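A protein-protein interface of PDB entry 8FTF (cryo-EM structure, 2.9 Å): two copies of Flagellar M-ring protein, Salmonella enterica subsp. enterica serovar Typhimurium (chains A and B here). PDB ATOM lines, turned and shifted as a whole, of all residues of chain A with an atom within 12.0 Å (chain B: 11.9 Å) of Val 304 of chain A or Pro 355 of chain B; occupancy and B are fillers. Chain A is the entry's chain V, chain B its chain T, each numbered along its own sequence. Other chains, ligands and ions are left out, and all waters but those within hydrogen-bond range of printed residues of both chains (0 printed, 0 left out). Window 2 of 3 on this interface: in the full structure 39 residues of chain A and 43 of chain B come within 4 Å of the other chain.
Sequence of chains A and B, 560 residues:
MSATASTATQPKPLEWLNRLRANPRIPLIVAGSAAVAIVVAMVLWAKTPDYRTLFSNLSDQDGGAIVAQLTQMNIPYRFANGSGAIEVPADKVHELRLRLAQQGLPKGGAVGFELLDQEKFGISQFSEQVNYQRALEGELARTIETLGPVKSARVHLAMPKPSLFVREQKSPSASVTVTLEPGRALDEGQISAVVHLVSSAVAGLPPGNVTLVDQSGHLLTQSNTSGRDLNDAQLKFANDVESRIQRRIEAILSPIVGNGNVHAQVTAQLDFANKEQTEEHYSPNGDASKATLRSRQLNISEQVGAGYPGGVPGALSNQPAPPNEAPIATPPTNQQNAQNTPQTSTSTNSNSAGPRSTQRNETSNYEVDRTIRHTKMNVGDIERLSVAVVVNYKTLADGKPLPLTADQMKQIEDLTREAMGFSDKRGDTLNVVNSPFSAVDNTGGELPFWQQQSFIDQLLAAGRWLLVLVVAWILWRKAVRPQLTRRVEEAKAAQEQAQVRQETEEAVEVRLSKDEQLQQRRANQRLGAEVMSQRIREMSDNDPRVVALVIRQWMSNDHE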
ATOM      1  N   ILE A 300     -28.005 -21.719  27.762  1.00  0.00           N
ATOM      2  CA  ILE A 300     -27.121 -20.690  27.225  1.00  0.00           C
ATOM      3  C   ILE A 300     -27.671 -19.309  27.574  1.00  0.00           C
ATOM      4  O   ILE A 300     -28.880 -19.056  27.500  1.00  0.00           O
ATOM      5  CB  ILE A 300     -26.950 -20.834  25.700  1.00  0.00           C
ATOM      6  CG1 ILE A 300     -26.277 -22.156  25.338  1.00  0.00           C
ATOM      7  CG2 ILE A 300     -26.150 -19.673  25.129  1.00  0.00           C
ATOM      8  CD1 ILE A 300     -27.253 -23.255  25.030  1.00  0.00           C
ATOM      9  N   SER A 301     -26.772 -18.407  27.963  1.00  0.00           N
ATOM     10  CA  SER A 301     -27.113 -17.002  28.124  1.00  0.00           C
ATOM     11  C   SER A 301     -26.013 -16.167  27.487  1.00  0.00           C
ATOM     12  O   SER A 301     -24.824 -16.416  27.702  1.00  0.00           O
ATOM     13  CB  SER A 301     -27.294 -16.625  29.599  1.00  0.00           C
ATOM     14  OG  SER A 301     -27.552 -15.239  29.740  1.00  0.00           O
ATOM     15  N   GLU A 302     -26.419 -15.170  26.702  1.00  0.00           N
ATOM     16  CA  GLU A 302     -25.466 -14.416  25.895  1.00  0.00           C
ATOM     17  C   GLU A 302     -26.013 -13.028  25.578  1.00  0.00           C
ATOM     18  O   GLU A 302     -26.951 -12.891  24.787  1.00  0.00           O
ATOM     19  CB  GLU A 302     -25.148 -15.200  24.621  1.00  0.00           C
ATOM     20  CG  GLU A 302     -23.982 -14.679  23.801  1.00  0.00           C
ATOM     21  CD  GLU A 302     -24.373 -13.567  22.856  1.00  0.00           C
ATOM     22  OE1 GLU A 302     -25.542 -13.536  22.417  1.00  0.00           O
ATOM     23  OE2 GLU A 302     -23.504 -12.732  22.540  1.00  0.00           O
ATOM     24  N   GLN A 303     -25.437 -11.993  26.192  1.00  0.00           N
ATOM     25  CA  GLN A 303     -25.964 -10.630  26.083  1.00  0.00           C
ATOM     26  C   GLN A 303     -24.895  -9.684  25.532  1.00  0.00           C
ATOM     27  O   GLN A 303     -23.942  -9.293  26.207  1.00  0.00           O
ATOM     28  CB  GLN A 303     -26.477 -10.153  27.435  1.00  0.00           C
ATOM     29  CG  GLN A 303     -27.311 -11.173  28.187  1.00  0.00           C
ATOM     30  CD  GLN A 303     -28.008 -10.577  29.393  1.00  0.00           C
ATOM     31  OE1 GLN A 303     -27.656  -9.490  29.850  1.00  0.00           O
ATOM     32  NE2 GLN A 303     -29.000 -11.288  29.915  1.00  0.00           N
ATOM     33  N   VAL A 304     -25.074  -9.316  24.261  1.00  0.00           N
ATOM     34  CA  VAL A 304     -24.248  -8.277  23.658  1.00  0.00           C
ATOM     35  C   VAL A 304     -24.867  -6.911  23.922  1.00  0.00           C
ATOM     36  O   VAL A 304     -26.069  -6.701  23.717  1.00  0.00           O
ATOM     37  CB  VAL A 304     -24.074  -8.522  22.150  1.00  0.00           C
ATOM     38  CG1 VAL A 304     -23.478  -7.297  21.477  1.00  0.00           C
ATOM     39  CG2 VAL A 304     -23.187  -9.722  21.910  1.00  0.00           C
ATOM     40  N   GLY A 305     -24.047  -5.975  24.379  1.00  0.00           N
ATOM     41  CA  GLY A 305     -24.498  -4.616  24.599  1.00  0.00           C
ATOM     42  C   GLY A 305     -23.606  -3.633  23.874  1.00  0.00           C
ATOM     43  O   GLY A 305     -22.388  -3.814  23.786  1.00  0.00           O
ATOM     44  N   ALA A 306     -24.228  -2.579  23.349  1.00  0.00           N
ATOM     45  CA  ALA A 306     -23.528  -1.555  22.588  1.00  0.00           C
ATOM     46  C   ALA A 306     -23.966  -0.177  23.058  1.00  0.00           C
ATOM     47  O   ALA A 306     -25.090  -0.003  23.535  1.00  0.00           O
ATOM     48  CB  ALA A 306     -23.789  -1.702  21.084  1.00  0.00           C
ATOM     49  N   GLY A 307     -23.071   0.796  22.920  1.00  0.00           N
ATOM     50  CA  GLY A 307     -23.361   2.161  23.319  1.00  0.00           C
ATOM     51  C   GLY A 307     -22.518   2.640  24.484  1.00  0.00           C
ATOM     52  O   GLY A 307     -22.724   3.739  25.002  1.00  0.00           O
ATOM     53  N   GLY A 354     -18.576  -3.745  23.111  1.00  0.00           N
ATOM     54  CA  GLY A 354     -19.188  -3.512  24.405  1.00  0.00           C
ATOM     55  C   GLY A 354     -19.212  -4.744  25.288  1.00  0.00           C
ATOM     56  O   GLY A 354     -18.497  -5.710  25.024  1.00  0.00           O
ATOM     57  N   PRO A 355     -20.024  -4.709  26.343  1.00  0.00           N
ATOM     58  CA  PRO A 355     -20.112  -5.862  27.246  1.00  0.00           C
ATOM     59  C   PRO A 355     -20.601  -7.109  26.524  1.00  0.00           C
ATOM     60  O   PRO A 355     -21.445  -7.044  25.629  1.00  0.00           O
ATOM     61  CB  PRO A 355     -21.114  -5.402  28.310  1.00  0.00           C
ATOM     62  CG  PRO A 355     -21.043  -3.910  28.276  1.00  0.00           C
ATOM     63  CD  PRO A 355     -20.785  -3.551  26.843  1.00  0.00           C
ATOM     64  N   ARG A 356     -20.050  -8.261  26.926  1.00  0.00           N
ATOM     65  CA  ARG A 356     -20.427  -9.572  26.389  1.00  0.00           C
ATOM     66  C   ARG A 356     -20.475 -10.546  27.565  1.00  0.00           C
ATOM     67  O   ARG A 356     -19.454 -11.117  27.956  1.00  0.00           O
ATOM     68  CB  ARG A 356     -19.454 -10.031  25.306  1.00  0.00           C
ATOM     69  CG  ARG A 356     -19.453  -9.169  24.054  1.00  0.00           C
ATOM     70  CD  ARG A 356     -18.446  -9.676  23.039  1.00  0.00           C
ATOM     71  NE  ARG A 356     -18.815 -10.984  22.510  1.00  0.00           N
ATOM     72  CZ  ARG A 356     -18.173 -12.111  22.782  1.00  0.00           C
ATOM     73  NH1 ARG A 356     -17.119 -12.129  23.582  1.00  0.00           N
ATOM     74  NH2 ARG A 356     -18.601 -13.249  22.243  1.00  0.00           N
ATOM     75  N   SER A 357     -21.669 -10.734  28.127  1.00  0.00           N
ATOM     76  CA  SER A 357     -21.846 -11.572  29.314  1.00  0.00           C
ATOM     77  C   SER A 357     -22.295 -12.974  28.897  1.00  0.00           C
ATOM     78  O   SER A 357     -23.454 -13.369  29.032  1.00  0.00           O
ATOM     79  CB  SER A 357     -22.838 -10.931  30.273  1.00  0.00           C
ATOM     80  OG  SER A 357     -22.556  -9.554  30.450  1.00  0.00           O
ATOM     81  N   THR A 358     -21.337 -13.736  28.379  1.00  0.00           N
ATOM     82  CA  THR A 358     -21.588 -15.128  28.035  1.00  0.00           C
ATOM     83  C   THR A 358     -21.724 -15.965  29.304  1.00  0.00           C
ATOM     84  O   THR A 358     -21.059 -15.715  30.313  1.00  0.00           O
ATOM     85  CB  THR A 358     -20.459 -15.667  27.154  1.00  0.00           C
ATOM     86  OG1 THR A 358     -20.334 -14.848  25.985  1.00  0.00           O
ATOM     87  CG2 THR A 358     -20.739 -17.099  26.720  1.00  0.00           C
ATOM     88  N   GLN A 359     -22.598 -16.967  29.248  1.00  0.00           N
ATOM     89  CA  GLN A 359     -22.846 -17.831  30.393  1.00  0.00           C
ATOM     90  C   GLN A 359     -23.308 -19.192  29.895  1.00  0.00           C
ATOM     91  O   GLN A 359     -24.043 -19.279  28.909  1.00  0.00           O
ATOM     92  CB  GLN A 359     -23.885 -17.211  31.335  1.00  0.00           C
ATOM     93  CG  GLN A 359     -24.479 -18.168  32.353  1.00  0.00           C
ATOM     94  CD  GLN A 359     -25.109 -17.447  33.527  1.00  0.00           C
ATOM     95  OE1 GLN A 359     -25.068 -16.221  33.611  1.00  0.00           O
ATOM     96  NE2 GLN A 359     -25.700 -18.208  34.442  1.00  0.00           N
ATOM     97  N   SER B 301     -35.681 -17.244  23.913  1.00  0.00           N
ATOM     98  CA  SER B 301     -35.924 -15.835  24.188  1.00  0.00           C
ATOM     99  C   SER B 301     -34.919 -15.014  23.396  1.00  0.00           C
ATOM    100  O   SER B 301     -33.723 -15.318  23.383  1.00  0.00           O
ATOM    101  CB  SER B 301     -35.821 -15.521  25.685  1.00  0.00           C
ATOM    102  OG  SER B 301     -35.986 -14.134  25.924  1.00  0.00           O
ATOM    103  N   GLU B 302     -35.414 -13.968  22.736  1.00  0.00           N
ATOM    104  CA  GLU B 302     -34.587 -13.213  21.800  1.00  0.00           C
ATOM    105  C   GLU B 302     -35.118 -11.793  21.640  1.00  0.00           C
ATOM    106  O   GLU B 302     -36.175 -11.584  21.037  1.00  0.00           O
ATOM    107  CB  GLU B 302     -34.536 -13.950  20.459  1.00  0.00           C
ATOM    108  CG  GLU B 302     -33.513 -13.436  19.462  1.00  0.00           C
ATOM    109  CD  GLU B 302     -34.017 -12.267  18.647  1.00  0.00           C
ATOM    110  OE1 GLU B 302     -35.243 -12.172  18.429  1.00  0.00           O
ATOM    111  OE2 GLU B 302     -33.181 -11.452  18.212  1.00  0.00           O
ATOM    112  N   GLN B 303     -34.394 -10.810  22.179  1.00  0.00           N
ATOM    113  CA  GLN B 303     -34.870  -9.424  22.220  1.00  0.00           C
ATOM    114  C   GLN B 303     -33.875  -8.496  21.521  1.00  0.00           C
ATOM    115  O   GLN B 303     -32.800  -8.171  22.029  1.00  0.00           O
ATOM    116  CB  GLN B 303     -35.111  -8.991  23.660  1.00  0.00           C
ATOM    117  CG  GLN B 303     -35.842 -10.013  24.509  1.00  0.00           C
ATOM    118  CD  GLN B 303     -36.285  -9.447  25.844  1.00  0.00           C
ATOM    119  OE1 GLN B 303     -35.808  -8.396  26.273  1.00  0.00           O
ATOM    120  NE2 GLN B 303     -37.198 -10.143  26.510  1.00  0.00           N
ATOM    121  N   VAL B 304     -34.262  -8.063  20.319  1.00  0.00           N
ATOM    122  CA  VAL B 304     -33.509  -7.029  19.618  1.00  0.00           C
ATOM    123  C   VAL B 304     -34.009  -5.653  20.042  1.00  0.00           C
ATOM    124  O   VAL B 304     -35.218  -5.389  20.066  1.00  0.00           O
ATOM    125  CB  VAL B 304     -33.620  -7.210  18.094  1.00  0.00           C
ATOM    126  CG1 VAL B 304     -33.098  -5.979  17.372  1.00  0.00           C
ATOM    127  CG2 VAL B 304     -32.845  -8.431  17.653  1.00  0.00           C
ATOM    128  N   GLY B 305     -33.079  -4.771  20.379  1.00  0.00           N
ATOM    129  CA  GLY B 305     -33.421  -3.408  20.729  1.00  0.00           C
ATOM    130  C   GLY B 305     -32.629  -2.427  19.893  1.00  0.00           C
ATOM    131  O   GLY B 305     -31.456  -2.650  19.580  1.00  0.00           O
ATOM    132  N   ALA B 306     -33.286  -1.327  19.530  1.00  0.00           N
ATOM    133  CA  ALA B 306     -32.688  -0.297  18.695  1.00  0.00           C
ATOM    134  C   ALA B 306     -32.972   1.074  19.290  1.00  0.00           C
ATOM    135  O   ALA B 306     -33.984   1.269  19.968  1.00  0.00           O
ATOM    136  CB  ALA B 306     -33.220  -0.364  17.259  1.00  0.00           C
ATOM    137  N   GLY B 307     -32.073   2.018  19.030  1.00  0.00           N
ATOM    138  CA  GLY B 307     -32.225   3.373  19.528  1.00  0.00           C
ATOM    139  C   GLY B 307     -31.165   3.766  20.539  1.00  0.00           C
ATOM    140  O   GLY B 307     -31.226   4.846  21.127  1.00  0.00           O
ATOM    141  N   GLY B 354     -27.827  -2.694  18.231  1.00  0.00           N
ATOM    142  CA  GLY B 354     -28.186  -2.498  19.622  1.00  0.00           C
ATOM    143  C   GLY B 354     -28.107  -3.768  20.447  1.00  0.00           C
ATOM    144  O   GLY B 354     -27.496  -4.747  20.020  1.00  0.00           O
ATOM    145  N   PRO B 355     -28.715  -3.750  21.631  1.00  0.00           N
ATOM    146  CA  PRO B 355     -28.692  -4.939  22.491  1.00  0.00           C
ATOM    147  C   PRO B 355     -29.359  -6.133  21.820  1.00  0.00           C
ATOM    148  O   PRO B 355     -30.346  -5.995  21.096  1.00  0.00           O
ATOM    149  CB  PRO B 355     -29.466  -4.492  23.735  1.00  0.00           C
ATOM    150  CG  PRO B 355     -29.335  -3.003  23.747  1.00  0.00           C
ATOM    151  CD  PRO B 355     -29.321  -2.588  22.305  1.00  0.00           C
ATOM    152  N   ARG B 356     -28.798  -7.322  22.072  1.00  0.00           N
ATOM    153  CA  ARG B 356     -29.325  -8.591  21.563  1.00  0.00           C
ATOM    154  C   ARG B 356     -29.206  -9.616  22.688  1.00  0.00           C
ATOM    155  O   ARG B 356     -28.158 -10.243  22.867  1.00  0.00           O
ATOM    156  CB  ARG B 356     -28.582  -9.037  20.304  1.00  0.00           C
ATOM    157  CG  ARG B 356     -28.767  -8.118  19.106  1.00  0.00           C
ATOM    158  CD  ARG B 356     -27.981  -8.616  17.907  1.00  0.00           C
ATOM    159  NE  ARG B 356     -28.498  -9.883  17.404  1.00  0.00           N
ATOM    160  CZ  ARG B 356     -27.869 -11.045  17.512  1.00  0.00           C
ATOM    161  NH1 ARG B 356     -26.692 -11.139  18.106  1.00  0.00           N
ATOM    162  NH2 ARG B 356     -28.438 -12.140  17.014  1.00  0.00           N
ATOM    163  N   SER B 357     -30.288  -9.785  23.449  1.00  0.00           N
ATOM    164  CA  SER B 357     -30.287 -10.670  24.615  1.00  0.00           C
ATOM    165  C   SER B 357     -30.867 -12.033  24.233  1.00  0.00           C
ATOM    166  O   SER B 357     -32.000 -12.389  24.560  1.00  0.00           O
ATOM    167  CB  SER B 357     -31.061 -10.036  25.762  1.00  0.00           C
ATOM    168  OG  SER B 357     -30.690  -8.681  25.937  1.00  0.00           O
ATOM    169  N   THR B 358     -30.052 -12.806  23.521  1.00  0.00           N
ATOM    170  CA  THR B 358     -30.425 -14.169  23.174  1.00  0.00           C
ATOM    171  C   THR B 358     -30.368 -15.059  24.414  1.00  0.00           C
ATOM    172  O   THR B 358     -29.523 -14.881  25.295  1.00  0.00           O
ATOM    173  CB  THR B 358     -29.497 -14.710  22.084  1.00  0.00           C
ATOM    174  OG1 THR B 358     -29.545 -13.843  20.944  1.00  0.00           O
ATOM    175  CG2 THR B 358     -29.915 -16.109  21.652  1.00  0.00           C
ATOM    176  N   GLN B 359     -31.283 -16.023  24.478  1.00  0.00           N
ATOM    177  CA  GLN B 359     -31.361 -16.930  25.615  1.00  0.00           C
ATOM    178  C   GLN B 359     -31.966 -18.247  25.157  1.00  0.00           C
ATOM    179  O   GLN B 359     -32.870 -18.262  24.316  1.00  0.00           O
ATOM    180  CB  GLN B 359     -32.186 -16.315  26.753  1.00  0.00           C
ATOM    181  CG  GLN B 359     -32.631 -17.294  27.823  1.00  0.00           C
ATOM    182  CD  GLN B 359     -33.009 -16.605  29.119  1.00  0.00           C
ATOM    183  OE1 GLN B 359     -32.898 -15.386  29.241  1.00  0.00           O
ATOM    184  NE2 GLN B 359     -33.459 -17.385  30.096  1.00  0.00           N
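Ile 300 of chain A touches Gln 359 of chain B (O to CA, 3.8 Å).
Arg 356 of chain B touches Gln 303 of chain A (O to CA, 3.9 Å).
O of Val 304 of chain A touches CA of Pro 355 of chain B (3.4 Å).
Val 304 of chain A touches two residues of chain B.
Of chain B, only Arg 356 (3.9 Å) comes within 4 Å of Gln 303 of chain A.
No residue of chain B comes within 4 Å of Gly 305 of chain A.
No residue of chain B comes within 4 Å of Ala 306 of chain A.
Gly 354 of chain A touches none of the printed residues of chain B.
No residue of chain B comes within 4 Å of Pro 355 of chain A.
No residue of chain B comes within 4 Å of Arg 356 of chain A.
No residue of chain B comes within 4 Å of Ser 357 of chain A.
No residue of chain A comes within 4 Å of Val 304 of chain B.
No residue of chain A comes within 4 Å of Gly 305 of chain B.
No residue of chain A comes within 4 Å of Ala 306 of chain B.
No residue of chain A comes within 4 Å of Gly 307 of chain B.
No residue of chain A comes within 4 Å of Gly 354 of chain B.
Of chain A, only Glu 302, Gln 303 and Val 304 come within 4 Å of Arg 356 of chain B.
Of the printed residues of chain B, Glu 302 of chain A touches Arg 356 and Thr 358.
Of the printed residues of chain A, Thr 358 of chain B touches Glu 302 (3.3 Å).
Printed residues of chain B within 4 Å of Ile 300 of chain A: Gln 359.
Of the printed residues of chain A, Gln 359 of chain B touches Ile 300 (3.8 Å).
Gln 359 of chain A touches none of the printed residues of chain B.
Glu 302 of chain B touches none of the printed residues of chain A.
The nearest residue of chain A that does not touch Pro 355 of chain B is Gly 305 of chain A (4.7 Å).
O of Val 304 of chain A sits at hydrogen-bond distance from N of Arg 356 of chain B, at 3.2 Å.
N of Thr 358 of chain B is in hydrogen-bond range of O of Glu 302 of chain A, at 3.4 Å.
The backbone carbonyl oxygen (O) of Glu 302 of chain A sits close to the backbone carbonyl oxygen (O) of Arg 356 of chain B (3.5 Å).
O of Ser 301 of chain B is in hydrogen-bond range of N of Gln 359 of chain B (2.8 Å).
O of Pro 355 of chain B is in hydrogen-bond range of N of Gly 305 of chain B (3.1 Å).
N of Ser 357 of chain A lies within hydrogen-bond range of O of Gln 303 of chain A, at 3.3 Å.
Glu 302 of chain A touches Arg 356 of chain B, but with the chains exchanged Arg 356 of chain A does not touch Glu 302 of chain B (15.0 Å).
Glu 302 of chain A touches Thr 358 of chain B, but with the chains exchanged Thr 358 of chain A does not touch Glu 302 of chain B (14.5 Å).
Gln 303 of chain A touches Arg 356 of chain B, but with the chains exchanged Arg 356 of chain A does not touch Gln 303 of chain B (13.2 Å).
Val 304 of chain A touches Pro 355 of chain B, but with the chains exchanged Pro 355 of chain A does not touch Val 304 of chain B (13.5 Å).
Of the 6 pairs that touch across the chains among the printed residues, none has its exchanged pair printed and touching as well.
Of the 14 printed residues of chain A, 4 touch a printed residue of chain B.
Printed residues of chain A that touch a printed residue of chain B: Ile 300, Glu 302, Gln 303 and Val 304.
Printed residues of chain B that touch a printed residue of chain A: Pro 355, Arg 356, Thr 358 and Gln 359.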
